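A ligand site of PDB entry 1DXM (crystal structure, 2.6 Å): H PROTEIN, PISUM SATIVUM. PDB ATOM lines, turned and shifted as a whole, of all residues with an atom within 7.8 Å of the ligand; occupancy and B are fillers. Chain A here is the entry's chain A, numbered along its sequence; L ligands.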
ATOM      1  N   PRO A  11     -19.917 -25.919 -12.723  1.00  0.00           N
ATOM      2  CA  PRO A  11     -20.381 -26.555 -11.481  1.00  0.00           C
ATOM      3  C   PRO A  11     -20.716 -25.542 -10.402  1.00  0.00           C
ATOM      4  O   PRO A  11     -21.543 -25.805  -9.526  1.00  0.00           O
ATOM      5  CB  PRO A  11     -19.181 -27.404 -11.087  1.00  0.00           C
ATOM      6  CG  PRO A  11     -18.575 -27.762 -12.403  1.00  0.00           C
ATOM      7  CD  PRO A  11     -18.620 -26.468 -13.148  1.00  0.00           C
ATOM      8  N   SER A  12     -20.050 -24.395 -10.437  1.00  0.00           N
ATOM      9  CA  SER A  12     -20.266 -23.333  -9.460  1.00  0.00           C
ATOM     10  C   SER A  12     -21.490 -22.493  -9.830  1.00  0.00           C
ATOM     11  O   SER A  12     -21.715 -21.411  -9.273  1.00  0.00           O
ATOM     12  CB  SER A  12     -19.012 -22.484  -9.297  1.00  0.00           C
ATOM     13  OG  SER A  12     -18.075 -22.733 -10.337  1.00  0.00           O
ATOM     14  N   HIS A  13     -22.273 -23.012 -10.772  1.00  0.00           N
ATOM     15  CA  HIS A  13     -23.517 -22.401 -11.260  1.00  0.00           C
ATOM     16  C   HIS A  13     -23.477 -21.155 -12.145  1.00  0.00           C
ATOM     17  O   HIS A  13     -24.462 -20.440 -12.241  1.00  0.00           O
ATOM     18  CB  HIS A  13     -24.484 -22.219 -10.101  1.00  0.00           C
ATOM     19  CG  HIS A  13     -24.728 -23.479  -9.339  1.00  0.00           C
ATOM     20  ND1 HIS A  13     -25.727 -24.368  -9.680  1.00  0.00           N
ATOM     21  CD2 HIS A  13     -24.053 -24.051  -8.316  1.00  0.00           C
ATOM     22  CE1 HIS A  13     -25.649 -25.432  -8.897  1.00  0.00           C
ATOM     23  NE2 HIS A  13     -24.642 -25.264  -8.063  1.00  0.00           N
ATOM     24  N   GLU A  14     -22.351 -20.905 -12.798  1.00  0.00           N
ATOM     25  CA  GLU A  14     -22.251 -19.776 -13.713  1.00  0.00           C
ATOM     26  C   GLU A  14     -22.497 -20.303 -15.120  1.00  0.00           C
ATOM     27  O   GLU A  14     -22.306 -21.495 -15.380  1.00  0.00           O
ATOM     28  CB  GLU A  14     -20.873 -19.100 -13.665  1.00  0.00           C
ATOM     29  CG  GLU A  14     -20.490 -18.496 -12.320  1.00  0.00           C
ATOM     30  CD  GLU A  14     -19.750 -19.468 -11.420  1.00  0.00           C
ATOM     31  OE1 GLU A  14     -19.596 -19.165 -10.221  1.00  0.00           O
ATOM     32  OE2 GLU A  14     -19.310 -20.524 -11.928  1.00  0.00           O
ATOM     33  N   ILE A  27     -24.941 -15.822 -13.630  1.00  0.00           N
ATOM     34  CA  ILE A  27     -25.199 -16.983 -12.787  1.00  0.00           C
ATOM     35  C   ILE A  27     -26.582 -17.553 -13.119  1.00  0.00           C
ATOM     36  O   ILE A  27     -27.498 -16.810 -13.495  1.00  0.00           O
ATOM     37  CB  ILE A  27     -25.074 -16.680 -11.278  1.00  0.00           C
ATOM     38  CG1 ILE A  27     -26.228 -15.807 -10.786  1.00  0.00           C
ATOM     39  CG2 ILE A  27     -23.738 -16.048 -10.989  1.00  0.00           C
ATOM     40  CD1 ILE A  27     -26.437 -15.849  -9.288  1.00  0.00           C
ATOM     41  N   THR A  28     -26.702 -18.866 -13.001  1.00  0.00           N
ATOM     42  CA  THR A  28     -27.949 -19.574 -13.302  1.00  0.00           C
ATOM     43  C   THR A  28     -29.139 -19.273 -12.391  1.00  0.00           C
ATOM     44  O   THR A  28     -29.009 -18.576 -11.382  1.00  0.00           O
ATOM     45  CB  THR A  28     -27.731 -21.091 -13.294  1.00  0.00           C
ATOM     46  OG1 THR A  28     -27.502 -21.517 -11.947  1.00  0.00           O
ATOM     47  CG2 THR A  28     -26.542 -21.455 -14.168  1.00  0.00           C
ATOM     48  N   HIS A  30     -30.823 -21.587 -10.789  1.00  0.00           N
ATOM     49  CA  HIS A  30     -30.682 -22.457  -9.615  1.00  0.00           C
ATOM     50  C   HIS A  30     -29.886 -21.707  -8.561  1.00  0.00           C
ATOM     51  O   HIS A  30     -30.195 -21.755  -7.370  1.00  0.00           O
ATOM     52  CB  HIS A  30     -29.963 -23.764  -9.989  1.00  0.00           C
ATOM     53  CG  HIS A  30     -29.622 -24.625  -8.821  1.00  0.00           C
ATOM     54  ND1 HIS A  30     -28.415 -24.537  -8.151  1.00  0.00           N
ATOM     55  CD2 HIS A  30     -30.336 -25.592  -8.187  1.00  0.00           C
ATOM     56  CE1 HIS A  30     -28.403 -25.414  -7.152  1.00  0.00           C
ATOM     57  NE2 HIS A  30     -29.549 -26.060  -7.152  1.00  0.00           N
ATOM     58  N   ALA A  31     -28.884 -20.960  -9.041  1.00  0.00           N
ATOM     59  CA  ALA A  31     -28.002 -20.184  -8.191  1.00  0.00           C
ATOM     60  C   ALA A  31     -28.737 -19.098  -7.415  1.00  0.00           C
ATOM     61  O   ALA A  31     -28.621 -19.051  -6.196  1.00  0.00           O
ATOM     62  CB  ALA A  31     -26.865 -19.586  -9.018  1.00  0.00           C
ATOM     63  N   GLN A  32     -29.507 -18.265  -8.118  1.00  0.00           N
ATOM     64  CA  GLN A  32     -30.233 -17.170  -7.478  1.00  0.00           C
ATOM     65  C   GLN A  32     -31.347 -17.674  -6.569  1.00  0.00           C
ATOM     66  O   GLN A  32     -31.656 -17.062  -5.551  1.00  0.00           O
ATOM     67  CB  GLN A  32     -30.765 -16.168  -8.513  1.00  0.00           C
ATOM     68  CG  GLN A  32     -31.887 -16.663  -9.430  1.00  0.00           C
ATOM     69  CD  GLN A  32     -33.230 -16.768  -8.727  1.00  0.00           C
ATOM     70  OE1 GLN A  32     -33.535 -15.979  -7.823  1.00  0.00           O
ATOM     71  NE2 GLN A  32     -34.026 -17.751  -9.109  1.00  0.00           N
ATOM     72  N   ASP A  33     -31.941 -18.793  -6.965  1.00  0.00           N
ATOM     73  CA  ASP A  33     -33.021 -19.411  -6.218  1.00  0.00           C
ATOM     74  C   ASP A  33     -32.465 -19.875  -4.873  1.00  0.00           C
ATOM     75  O   ASP A  33     -33.143 -19.823  -3.860  1.00  0.00           O
ATOM     76  CB  ASP A  33     -33.611 -20.578  -7.000  1.00  0.00           C
ATOM     77  CG  ASP A  33     -34.838 -21.168  -6.340  1.00  0.00           C
ATOM     78  OD1 ASP A  33     -35.827 -20.431  -6.128  1.00  0.00           O
ATOM     79  OD2 ASP A  33     -34.826 -22.374  -6.018  1.00  0.00           O
ATOM     80  N   HIS A  34     -31.209 -20.314  -4.886  1.00  0.00           N
ATOM     81  CA  HIS A  34     -30.558 -20.774  -3.668  1.00  0.00           C
ATOM     82  C   HIS A  34     -29.963 -19.619  -2.866  1.00  0.00           C
ATOM     83  O   HIS A  34     -29.944 -19.649  -1.634  1.00  0.00           O
ATOM     84  CB  HIS A  34     -29.508 -21.821  -3.988  1.00  0.00           C
ATOM     85  CG  HIS A  34     -30.086 -23.172  -4.286  1.00  0.00           C
ATOM     86  ND1 HIS A  34     -31.050 -23.357  -5.260  1.00  0.00           N
ATOM     87  CD2 HIS A  34     -29.892 -24.379  -3.711  1.00  0.00           C
ATOM     88  CE1 HIS A  34     -31.430 -24.625  -5.250  1.00  0.00           C
ATOM     89  NE2 HIS A  34     -30.744 -25.263  -4.322  1.00  0.00           N
ATOM     90  N   LEU A  35     -29.495 -18.588  -3.566  1.00  0.00           N
ATOM     91  CA  LEU A  35     -28.926 -17.439  -2.881  1.00  0.00           C
ATOM     92  C   LEU A  35     -29.951 -16.639  -2.108  1.00  0.00           C
ATOM     93  O   LEU A  35     -29.658 -16.100  -1.028  1.00  0.00           O
ATOM     94  CB  LEU A  35     -28.230 -16.508  -3.869  1.00  0.00           C
ATOM     95  CG  LEU A  35     -26.857 -16.909  -4.362  1.00  0.00           C
ATOM     96  CD1 LEU A  35     -26.327 -15.797  -5.228  1.00  0.00           C
ATOM     97  CD2 LEU A  35     -25.926 -17.158  -3.183  1.00  0.00           C
ATOM     98  N   GLY A  36     -31.166 -16.584  -2.635  1.00  0.00           N
ATOM     99  CA  GLY A  36     -32.213 -15.805  -2.008  1.00  0.00           C
ATOM    100  C   GLY A  36     -32.133 -14.405  -2.606  1.00  0.00           C
ATOM    101  O   GLY A  36     -31.368 -14.185  -3.560  1.00  0.00           O
ATOM    102  N   VAL A  59     -21.631 -11.794  -5.480  1.00  0.00           N
ATOM    103  CA  VAL A  59     -23.047 -11.542  -5.381  1.00  0.00           C
ATOM    104  C   VAL A  59     -23.370 -11.687  -3.909  1.00  0.00           C
ATOM    105  O   VAL A  59     -22.924 -12.641  -3.269  1.00  0.00           O
ATOM    106  CB  VAL A  59     -23.846 -12.594  -6.184  1.00  0.00           C
ATOM    107  CG1 VAL A  59     -25.329 -12.393  -5.997  1.00  0.00           C
ATOM    108  CG2 VAL A  59     -23.499 -12.514  -7.665  1.00  0.00           C
ATOM    109  N   GLU A  60     -24.038 -10.700  -3.342  1.00  0.00           N
ATOM    110  CA  GLU A  60     -24.422 -10.755  -1.933  1.00  0.00           C
ATOM    111  C   GLU A  60     -25.912 -10.899  -1.838  1.00  0.00           C
ATOM    112  O   GLU A  60     -26.659 -10.277  -2.586  1.00  0.00           O
ATOM    113  CB  GLU A  60     -24.017  -9.494  -1.162  1.00  0.00           C
ATOM    114  CG  GLU A  60     -22.554  -9.435  -0.698  1.00  0.00           C
ATOM    115  CD  GLU A  60     -21.605  -8.921  -1.762  1.00  0.00           C
ATOM    116  OE1 GLU A  60     -20.472  -9.439  -1.830  1.00  0.00           O
ATOM    117  OE2 GLU A  60     -21.967  -7.990  -2.514  1.00  0.00           O
ATOM    118  N   SER A  61     -26.347 -11.766  -0.935  1.00  0.00           N
ATOM    119  CA  SER A  61     -27.766 -11.966  -0.706  1.00  0.00           C
ATOM    120  C   SER A  61     -28.048 -11.475   0.695  1.00  0.00           C
ATOM    121  O   SER A  61     -27.170 -10.928   1.374  1.00  0.00           O
ATOM    122  CB  SER A  61     -28.114 -13.453  -0.807  1.00  0.00           C
ATOM    123  OG  SER A  61     -27.479 -14.194   0.214  1.00  0.00           O
ATOM    124  N   VAL A  62     -29.282 -11.657   1.134  1.00  0.00           N
ATOM    125  CA  VAL A  62     -29.664 -11.245   2.470  1.00  0.00           C
ATOM    126  C   VAL A  62     -28.967 -12.158   3.482  1.00  0.00           C
ATOM    127  O   VAL A  62     -28.812 -11.770   4.638  1.00  0.00           O
ATOM    128  CB  VAL A  62     -31.185 -11.259   2.648  1.00  0.00           C
ATOM    129  CG1 VAL A  62     -31.785 -10.054   1.922  1.00  0.00           C
ATOM    130  CG2 VAL A  62     -31.761 -12.541   2.072  1.00  0.00           C
ATOM    131  N   LYS A  63     -28.541 -13.356   3.069  1.00  0.00           N
ATOM    132  CA  LYS A  63     -27.831 -14.247   3.994  1.00  0.00           C
ATOM    133  C   LYS A  63     -26.318 -14.194   3.860  1.00  0.00           C
ATOM    134  O   LYS A  63     -25.617 -14.062   4.878  1.00  0.00           O
ATOM    135  CB  LYS A  63     -28.253 -15.741   3.947  1.00  0.00           C
ATOM    136  CG  LYS A  63     -29.269 -16.213   2.930  1.00  0.00           C
ATOM    137  CD  LYS A  63     -29.203 -17.762   2.908  1.00  0.00           C
ATOM    138  CE  LYS A  63     -29.264 -18.363   1.490  1.00  0.00           C
ATOM    139  NZ  LYS A  63     -28.280 -19.468   1.515  1.00  0.00           N
ATOM    140  N   ALA A  64     -25.807 -14.272   2.627  1.00  0.00           N
ATOM    141  CA  ALA A  64     -24.369 -14.286   2.453  1.00  0.00           C
ATOM    142  C   ALA A  64     -23.698 -13.691   1.205  1.00  0.00           C
ATOM    143  O   ALA A  64     -24.354 -13.119   0.323  1.00  0.00           O
ATOM    144  CB  ALA A  64     -23.873 -15.719   2.659  1.00  0.00           C
ATOM    145  N   THR A  65     -22.375 -13.785   1.211  1.00  0.00           N
ATOM    146  CA  THR A  65     -21.510 -13.332   0.136  1.00  0.00           C
ATOM    147  C   THR A  65     -21.134 -14.576  -0.663  1.00  0.00           C
ATOM    148  O   THR A  65     -20.607 -15.550  -0.112  1.00  0.00           O
ATOM    149  CB  THR A  65     -20.232 -12.732   0.689  1.00  0.00           C
ATOM    150  OG1 THR A  65     -20.567 -11.596   1.468  1.00  0.00           O
ATOM    151  CG2 THR A  65     -19.309 -12.321  -0.443  1.00  0.00           C
ATOM    152  N   SER A  66     -21.413 -14.530  -1.952  1.00  0.00           N
ATOM    153  CA  SER A  66     -21.139 -15.646  -2.844  1.00  0.00           C
ATOM    154  C   SER A  66     -20.230 -15.195  -3.989  1.00  0.00           C
ATOM    155  O   SER A  66     -20.652 -14.455  -4.874  1.00  0.00           O
ATOM    156  CB  SER A  66     -22.468 -16.176  -3.369  1.00  0.00           C
ATOM    157  OG  SER A  66     -22.312 -17.380  -4.081  1.00  0.00           O
ATOM    158  N   TYR A 120     -25.753 -30.178 -16.883  1.00  0.00           N
ATOM    159  CA  TYR A 120     -25.936 -29.296 -15.739  1.00  0.00           C
ATOM    160  C   TYR A 120     -27.149 -29.672 -14.895  1.00  0.00           C
ATOM    161  O   TYR A 120     -27.080 -29.659 -13.670  1.00  0.00           O
ATOM    162  CB  TYR A 120     -26.052 -27.832 -16.203  1.00  0.00           C
ATOM    163  CG  TYR A 120     -26.237 -26.809 -15.087  1.00  0.00           C
ATOM    164  CD1 TYR A 120     -25.186 -26.484 -14.232  1.00  0.00           C
ATOM    165  CD2 TYR A 120     -27.474 -26.181 -14.892  1.00  0.00           C
ATOM    166  CE1 TYR A 120     -25.347 -25.554 -13.205  1.00  0.00           C
ATOM    167  CE2 TYR A 120     -27.647 -25.257 -13.870  1.00  0.00           C
ATOM    168  CZ  TYR A 120     -26.584 -24.950 -13.038  1.00  0.00           C
ATOM    169  OH  TYR A 120     -26.740 -24.044 -12.011  1.00  0.00           O
ATOM    170  N   PHE A 123     -26.405 -32.489 -12.880  1.00  0.00           N
ATOM    171  CA  PHE A 123     -25.526 -31.997 -11.837  1.00  0.00           C
ATOM    172  C   PHE A 123     -26.335 -31.340 -10.722  1.00  0.00           C
ATOM    173  O   PHE A 123     -26.178 -31.700  -9.551  1.00  0.00           O
ATOM    174  CB  PHE A 123     -24.524 -30.991 -12.389  1.00  0.00           C
ATOM    175  CG  PHE A 123     -23.675 -30.351 -11.321  1.00  0.00           C
ATOM    176  CD1 PHE A 123     -22.656 -31.073 -10.716  1.00  0.00           C
ATOM    177  CD2 PHE A 123     -23.923 -29.058 -10.896  1.00  0.00           C
ATOM    178  CE1 PHE A 123     -21.898 -30.516  -9.692  1.00  0.00           C
ATOM    179  CE2 PHE A 123     -23.169 -28.488  -9.879  1.00  0.00           C
ATOM    180  CZ  PHE A 123     -22.160 -29.216  -9.280  1.00  0.00           C
ATOM    181  N   CYS A 124     -27.199 -30.388 -11.077  1.00  0.00           N
ATOM    182  CA  CYS A 124     -28.015 -29.712 -10.075  1.00  0.00           C
ATOM    183  C   CYS A 124     -28.867 -30.696  -9.301  1.00  0.00           C
ATOM    184  O   CYS A 124     -29.130 -30.491  -8.124  1.00  0.00           O
ATOM    185  CB  CYS A 124     -28.868 -28.606 -10.709  1.00  0.00           C
ATOM    186  SG  CYS A 124     -27.900 -27.166 -11.257  1.00  0.00           S
ATOM    187  N   GLU A 127     -26.506 -32.500  -6.629  1.00  0.00           N
ATOM    188  CA  GLU A 127     -26.185 -31.598  -5.540  1.00  0.00           C
ATOM    189  C   GLU A 127     -27.380 -31.382  -4.614  1.00  0.00           C
ATOM    190  O   GLU A 127     -27.220 -31.311  -3.387  1.00  0.00           O
ATOM    191  CB  GLU A 127     -25.688 -30.266  -6.130  1.00  0.00           C
ATOM    192  CG  GLU A 127     -24.872 -29.389  -5.186  1.00  0.00           C
ATOM    193  CD  GLU A 127     -24.292 -28.167  -5.880  1.00  0.00           C
ATOM    194  OE1 GLU A 127     -24.718 -27.858  -7.015  1.00  0.00           O
ATOM    195  OE2 GLU A 127     -23.394 -27.515  -5.304  1.00  0.00           O
ATOM    196  N   ASP A 128     -28.571 -31.275  -5.194  1.00  0.00           N
ATOM    197  CA  ASP A 128     -29.792 -31.090  -4.415  1.00  0.00           C
ATOM    198  C   ASP A 128     -30.139 -32.369  -3.652  1.00  0.00           C
ATOM    199  O   ASP A 128     -30.679 -32.318  -2.544  1.00  0.00           O
ATOM    200  CB  ASP A 128     -30.975 -30.720  -5.317  1.00  0.00           C
ATOM    201  CG  ASP A 128     -30.866 -29.310  -5.898  1.00  0.00           C
ATOM    202  OD1 ASP A 128     -30.299 -28.415  -5.234  1.00  0.00           O
ATOM    203  OD2 ASP A 128     -31.362 -29.102  -7.030  1.00  0.00           O
HETATM  204  C1  LIG L   1     -27.110 -19.123   0.920  1.00  0.00           C
HETATM  205  O1  LIG L   1     -26.913 -17.999   0.456  1.00  0.00           O
HETATM  206  C2  LIG L   1     -26.026 -20.172   0.803  1.00  0.00           C
HETATM  207  C3  LIG L   1     -25.273 -20.070  -0.534  1.00  0.00           C
HETATM  208  C4  LIG L   1     -26.099 -20.637  -1.691  1.00  0.00           C
HETATM  209  C5  LIG L   1     -25.335 -20.616  -3.016  1.00  0.00           C
HETATM  210  C6  LIG L   1     -25.820 -21.659  -4.026  1.00  0.00           C
HETATM  211  C7  LIG L   1     -25.722 -23.075  -3.452  1.00  0.00           C
HETATM  212  C8  LIG L   1     -26.023 -24.158  -4.473  1.00  0.00           C
HETATM  213  S1  LIG L   1     -26.179 -25.803  -3.772  1.00  0.00           S
HETATM  214  S2  LIG L   1     -25.074 -21.518  -5.662  1.00  0.00           S
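Residues that only touch the ligand: His 13 (3.8 Å), His 30 (3.8 Å), His 34 (3.7 Å), Leu 35 (3.5 Å) and Ser 61 (3.9 Å).
Hydrophobic or aromatic side chains that line the ligand: His 13, His 30, His 34 and Leu 35.
The nearest printed residue that does not touch the ligand is Ala 31 (4.1 Å).
NZ of Lys 63 is covalently linked to C1 of the ligand.
OE2 of Glu 127 lies close to S1 of the ligand, 3.6 Å away.
The backbone carbonyl oxygen (O) of Pro 11 sits close to a ring nitrogen (NE2) of His 13 (3.5 Å).
The side-chain hydroxyl (OG) of Ser 61 lies close to the backbone NH (N) of Lys 63.
A ring nitrogen (NE2) of His 30 lies within hydrogen-bond range of the side-chain carboxylate of Asp 128 (3.1 Å).
A ring nitrogen (ND1) of His 34 sits at hydrogen-bond distance from the backbone carbonyl oxygen (O) of His 30, at 2.8 Å.
A ring nitrogen (ND1) of His 13 lies within hydrogen-bond range of the side-chain hydroxyl (OH) of Tyr 120.
The side-chain hydroxyl of Ser 61 sits at hydrogen-bond distance from the backbone NH of Ala 64 (2.9 Å).
A ring nitrogen (ND1) of His 30 lies close to a ring nitrogen (ND1) of His 13, at 3.1 Å.
O of His 13 is in hydrogen-bond range of N of Thr 28 (2.8 Å).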
